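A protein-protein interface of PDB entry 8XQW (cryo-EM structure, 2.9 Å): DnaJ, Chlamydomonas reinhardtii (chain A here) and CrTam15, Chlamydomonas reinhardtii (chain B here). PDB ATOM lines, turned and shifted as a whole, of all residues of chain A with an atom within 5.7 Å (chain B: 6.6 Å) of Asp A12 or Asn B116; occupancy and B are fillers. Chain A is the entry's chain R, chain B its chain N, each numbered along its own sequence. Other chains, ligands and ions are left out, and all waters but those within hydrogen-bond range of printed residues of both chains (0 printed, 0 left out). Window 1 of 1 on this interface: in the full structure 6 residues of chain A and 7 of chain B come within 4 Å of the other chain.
Asp A12 touches just these residues of chain B: Tyr B114, Gly B115, Asn B116 and Met B117.
Printed residues of chain A within 4 Å of Asn B116: Asp A10 (3.98 Å), Gly A11 (2.9 Å) and Asp A12 (3.5 Å).
Printed residues of chain A within 4 Å of Gly B115: Asp A12.
Printed residues of chain B within 4 Å of Gly A11: Asn B116.
Of the printed residues of chain A, Asp B118 touches Asp A10 (2.5 Å).
Gly B112 touches none of the printed residues of chain A.
Asp A16 touches none of the printed residues of chain B.
The nearest residue of chain B that does not touch Asp A12 is Arg B113 (4.8 Å).
The nearest printed residue of chain B that does not touch Asp A10 is Gly B119 (4.8 Å).
Of the 10 printed residues of chain B, 6 touch a printed residue of chain A.
Printed residues of chain B that touch a printed residue of chain A: Arg B113, Tyr B114, Gly B115, Asn B116, Met B117 and Asp B118.
Hydrophobic or aromatic side chains of chain B within 4 Å of the printed part of chain A: Tyr B114 and Met B117.
Of the 8 printed residues of chain A, 5 touch a printed residue of chain B.
Hydrophobic or aromatic side chains of chain A that line the printed part of chain B: Pro A13.
Among the printed residues, 11 pairs touch across the chains.
Among the printed residues, pairs that only touch across the chains: Asp A10 with Met B117 (3.3 Å), Asp A12 with Tyr B114 (3.5 Å), Asp A12 with Asn B116 (3.5 Å), Asp A12 with Met B117 (3.6 Å), Pro A13 with Arg B113 (3.7 Å), Pro A13 with Tyr B114 (3.8 Å), Asp A10 with Asn B116 (3.98 Å) and Phe A9 with Met B117 (3.999 Å).
NH2 of Arg B113 is in hydrogen-bond range of OH of Tyr B114, 3.2 Å away.
OD1 of Asp A12 sits at hydrogen-bond distance from N of Val A15, at 3.4 Å.
O of Pro A13 sits close to OD1 of Asp A16 (2.7 Å).
The backbone NH (N) of Tyr A14 is in hydrogen-bond range of the side-chain carboxylate (OD1) of Asp A12, 2.7 Å away.
N of Asp B118 lies within hydrogen-bond range of O of Asp A10 (2.5 Å).
The side-chain carboxylate of Asp A12 is in hydrogen-bond range of the backbone NH of Gly B115 (2.6 Å).
The backbone carbonyl oxygen of Gly A11 lies close to the backbone carbonyl oxygen of Asn B116, at 2.9 Å.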
ATOM      1  N   PHE A   9       9.026  27.384  -4.098  1.00  0.00           N
ATOM      2  CA  PHE A   9       7.708  26.705  -3.974  1.00  0.00           C
ATOM      3  C   PHE A   9       7.851  25.336  -3.347  1.00  0.00           C
ATOM      4  O   PHE A   9       6.922  24.537  -3.515  1.00  0.00           O
ATOM      5  CB  PHE A   9       7.006  26.675  -5.332  1.00  0.00           C
ATOM      6  CG  PHE A   9       6.652  28.061  -5.850  1.00  0.00           C
ATOM      7  CD1 PHE A   9       7.438  28.685  -6.809  1.00  0.00           C
ATOM      8  CD2 PHE A   9       5.550  28.744  -5.356  1.00  0.00           C
ATOM      9  CE1 PHE A   9       7.118  29.950  -7.268  1.00  0.00           C
ATOM     10  CE2 PHE A   9       5.235  30.009  -5.819  1.00  0.00           C
ATOM     11  CZ  PHE A   9       6.021  30.609  -6.772  1.00  0.00           C
ATOM     12  N   ASP A  10       8.960  25.049  -2.665  1.00  0.00           N
ATOM     13  CA  ASP A  10       9.067  23.808  -1.919  1.00  0.00           C
ATOM     14  C   ASP A  10       8.452  23.968  -0.537  1.00  0.00           C
ATOM     15  O   ASP A  10       8.479  25.045   0.061  1.00  0.00           O
ATOM     16  CB  ASP A  10      10.528  23.380  -1.796  1.00  0.00           C
ATOM     17  CG  ASP A  10      11.246  23.372  -3.130  1.00  0.00           C
ATOM     18  OD1 ASP A  10      11.286  24.429  -3.794  1.00  0.00           O
ATOM     19  OD2 ASP A  10      11.769  22.305  -3.516  1.00  0.00           O
ATOM     20  N   GLY A  11       7.883  22.879  -0.029  1.00  0.00           N
ATOM     21  CA  GLY A  11       7.326  22.862   1.306  1.00  0.00           C
ATOM     22  C   GLY A  11       5.820  22.758   1.377  1.00  0.00           C
ATOM     23  O   GLY A  11       5.278  22.689   2.486  1.00  0.00           O
ATOM     24  N   ASP A  12       5.124  22.742   0.245  1.00  0.00           N
ATOM     25  CA  ASP A  12       3.675  22.592   0.226  1.00  0.00           C
ATOM     26  C   ASP A  12       3.339  21.277  -0.457  1.00  0.00           C
ATOM     27  O   ASP A  12       3.774  21.049  -1.599  1.00  0.00           O
ATOM     28  CB  ASP A  12       3.006  23.767  -0.488  1.00  0.00           C
ATOM     29  CG  ASP A  12       1.489  23.703  -0.441  1.00  0.00           C
ATOM     30  OD1 ASP A  12       0.903  22.765  -1.018  1.00  0.00           O
ATOM     31  OD2 ASP A  12       0.878  24.598   0.177  1.00  0.00           O
ATOM     32  N   PRO A  13       2.583  20.387   0.185  1.00  0.00           N
ATOM     33  CA  PRO A  13       2.331  19.072  -0.420  1.00  0.00           C
ATOM     34  C   PRO A  13       1.522  19.133  -1.700  1.00  0.00           C
ATOM     35  O   PRO A  13       1.407  18.117  -2.392  1.00  0.00           O
ATOM     36  CB  PRO A  13       1.573  18.322   0.684  1.00  0.00           C
ATOM     37  CG  PRO A  13       1.837  19.079   1.926  1.00  0.00           C
ATOM     38  CD  PRO A  13       1.988  20.500   1.522  1.00  0.00           C
ATOM     39  N   TYR A  14       0.944  20.278  -2.042  1.00  0.00           N
ATOM     40  CA  TYR A  14       0.093  20.331  -3.217  1.00  0.00           C
ATOM     41  C   TYR A  14       0.769  20.951  -4.427  1.00  0.00           C
ATOM     42  O   TYR A  14       0.435  20.583  -5.556  1.00  0.00           O
ATOM     43  CB  TYR A  14      -1.189  21.101  -2.912  1.00  0.00           C
ATOM     44  CG  TYR A  14      -2.243  20.928  -3.969  1.00  0.00           C
ATOM     45  CD1 TYR A  14      -3.047  19.803  -3.991  1.00  0.00           C
ATOM     46  CD2 TYR A  14      -2.428  21.884  -4.952  1.00  0.00           C
ATOM     47  CE1 TYR A  14      -4.008  19.640  -4.960  1.00  0.00           C
ATOM     48  CE2 TYR A  14      -3.385  21.730  -5.924  1.00  0.00           C
ATOM     49  CZ  TYR A  14      -4.173  20.607  -5.924  1.00  0.00           C
ATOM     50  OH  TYR A  14      -5.129  20.450  -6.896  1.00  0.00           O
ATOM     51  N   VAL A  15       1.704  21.879  -4.227  1.00  0.00           N
ATOM     52  CA  VAL A  15       2.349  22.525  -5.365  1.00  0.00           C
ATOM     53  C   VAL A  15       3.215  21.527  -6.120  1.00  0.00           C
ATOM     54  O   VAL A  15       3.358  21.608  -7.346  1.00  0.00           O
ATOM     55  CB  VAL A  15       3.160  23.746  -4.898  1.00  0.00           C
ATOM     56  CG1 VAL A  15       4.109  23.349  -3.802  1.00  0.00           C
ATOM     57  CG2 VAL A  15       3.920  24.366  -6.057  1.00  0.00           C
ATOM     58  N   ASP A  16       3.794  20.560  -5.409  1.00  0.00           N
ATOM     59  CA  ASP A  16       4.612  19.561  -6.083  1.00  0.00           C
ATOM     60  C   ASP A  16       3.783  18.656  -6.981  1.00  0.00           C
ATOM     61  O   ASP A  16       4.244  18.283  -8.063  1.00  0.00           O
ATOM     62  CB  ASP A  16       5.387  18.728  -5.062  1.00  0.00           C
ATOM     63  CG  ASP A  16       4.486  18.026  -4.062  1.00  0.00           C
ATOM     64  OD1 ASP A  16       3.285  17.845  -4.347  1.00  0.00           O
ATOM     65  OD2 ASP A  16       4.985  17.656  -2.979  1.00  0.00           O
ATOM     66  N   PRO B 111       0.190  27.972  12.242  1.00  0.00           N
ATOM     67  CA  PRO B 111       0.068  27.491  10.864  1.00  0.00           C
ATOM     68  C   PRO B 111      -0.233  26.001  10.798  1.00  0.00           C
ATOM     69  O   PRO B 111      -0.210  25.283  11.799  1.00  0.00           O
ATOM     70  CB  PRO B 111       1.441  27.802  10.255  1.00  0.00           C
ATOM     71  CG  PRO B 111       2.091  28.751  11.207  1.00  0.00           C
ATOM     72  CD  PRO B 111       1.568  28.386  12.545  1.00  0.00           C
ATOM     73  N   GLY B 112      -0.523  25.539   9.583  1.00  0.00           N
ATOM     74  CA  GLY B 112      -0.835  24.144   9.346  1.00  0.00           C
ATOM     75  C   GLY B 112       0.200  23.434   8.499  1.00  0.00           C
ATOM     76  O   GLY B 112       1.402  23.571   8.740  1.00  0.00           O
ATOM     77  N   ARG B 113      -0.249  22.671   7.501  1.00  0.00           N
ATOM     78  CA  ARG B 113       0.661  21.969   6.609  1.00  0.00           C
ATOM     79  C   ARG B 113       0.734  22.566   5.215  1.00  0.00           C
ATOM     80  O   ARG B 113       1.794  22.491   4.587  1.00  0.00           O
ATOM     81  CB  ARG B 113       0.266  20.492   6.480  1.00  0.00           C
ATOM     82  CG  ARG B 113       0.275  19.734   7.788  1.00  0.00           C
ATOM     83  CD  ARG B 113       0.293  18.235   7.555  1.00  0.00           C
ATOM     84  NE  ARG B 113      -0.530  17.839   6.416  1.00  0.00           N
ATOM     85  CZ  ARG B 113      -0.955  16.598   6.194  1.00  0.00           C
ATOM     86  NH1 ARG B 113      -0.645  15.624   7.038  1.00  0.00           N
ATOM     87  NH2 ARG B 113      -1.696  16.331   5.128  1.00  0.00           N
ATOM     88  N   TYR B 114      -0.346  23.148   4.720  1.00  0.00           N
ATOM     89  CA  TYR B 114      -0.364  23.739   3.394  1.00  0.00           C
ATOM     90  C   TYR B 114      -0.142  25.242   3.487  1.00  0.00           C
ATOM     91  O   TYR B 114      -0.115  25.824   4.571  1.00  0.00           O
ATOM     92  CB  TYR B 114      -1.685  23.440   2.683  1.00  0.00           C
ATOM     93  CG  TYR B 114      -2.076  21.980   2.718  1.00  0.00           C
ATOM     94  CD1 TYR B 114      -2.722  21.443   3.817  1.00  0.00           C
ATOM     95  CD2 TYR B 114      -1.802  21.142   1.650  1.00  0.00           C
ATOM     96  CE1 TYR B 114      -3.082  20.117   3.855  1.00  0.00           C
ATOM     97  CE2 TYR B 114      -2.162  19.813   1.678  1.00  0.00           C
ATOM     98  CZ  TYR B 114      -2.800  19.307   2.785  1.00  0.00           C
ATOM     99  OH  TYR B 114      -3.163  17.984   2.830  1.00  0.00           O
ATOM    100  N   GLY B 115       0.031  25.864   2.328  1.00  0.00           N
ATOM    101  CA  GLY B 115       0.282  27.285   2.279  1.00  0.00           C
ATOM    102  C   GLY B 115       1.636  27.714   2.790  1.00  0.00           C
ATOM    103  O   GLY B 115       1.877  28.918   2.922  1.00  0.00           O
ATOM    104  N   ASN B 116       2.527  26.775   3.075  1.00  0.00           N
ATOM    105  CA  ASN B 116       3.849  27.073   3.614  1.00  0.00           C
ATOM    106  C   ASN B 116       4.885  26.764   2.540  1.00  0.00           C
ATOM    107  O   ASN B 116       5.248  25.608   2.321  1.00  0.00           O
ATOM    108  CB  ASN B 116       4.107  26.275   4.879  1.00  0.00           C
ATOM    109  CG  ASN B 116       4.951  27.031   5.873  1.00  0.00           C
ATOM    110  OD1 ASN B 116       5.877  27.747   5.497  1.00  0.00           O
ATOM    111  ND2 ASN B 116       4.632  26.885   7.153  1.00  0.00           N
ATOM    112  N   MET B 117       5.355  27.805   1.860  1.00  0.00           N
ATOM    113  CA  MET B 117       6.409  27.664   0.870  1.00  0.00           C
ATOM    114  C   MET B 117       7.759  27.950   1.510  1.00  0.00           C
ATOM    115  O   MET B 117       7.853  28.722   2.468  1.00  0.00           O
ATOM    116  CB  MET B 117       6.182  28.611  -0.309  1.00  0.00           C
ATOM    117  CG  MET B 117       4.784  28.567  -0.891  1.00  0.00           C
ATOM    118  SD  MET B 117       4.380  26.978  -1.625  1.00  0.00           S
ATOM    119  CE  MET B 117       2.605  27.124  -1.776  1.00  0.00           C
ATOM    120  N   ASP B 118       8.804  27.319   0.981  1.00  0.00           N
ATOM    121  CA  ASP B 118      10.147  27.583   1.486  1.00  0.00           C
ATOM    122  C   ASP B 118      10.692  28.913   0.990  1.00  0.00           C
ATOM    123  O   ASP B 118      11.739  29.359   1.470  1.00  0.00           O
ATOM    124  CB  ASP B 118      11.095  26.454   1.088  1.00  0.00           C
ATOM    125  CG  ASP B 118      12.054  26.085   2.197  1.00  0.00           C
ATOM    126  OD1 ASP B 118      12.588  27.003   2.856  1.00  0.00           O
ATOM    127  OD2 ASP B 118      12.272  24.874   2.413  1.00  0.00           O
ATOM    128  N   GLY B 119      10.018  29.549   0.039  1.00  0.00           N
ATOM    129  CA  GLY B 119      10.454  30.840  -0.442  1.00  0.00           C
ATOM    130  C   GLY B 119       9.742  31.983   0.243  1.00  0.00           C
ATOM    131  O   GLY B 119       9.914  33.146  -0.131  1.00  0.00           O
ATOM    132  N   GLY B 120       8.936  31.663   1.257  1.00  0.00           N
ATOM    133  CA  GLY B 120       8.173  32.691   1.937  1.00  0.00           C
ATOM    134  C   GLY B 120       8.961  33.454   2.978  1.00  0.00           C
ATOM    135  O   GLY B 120       8.788  34.668   3.117  1.00  0.00           O
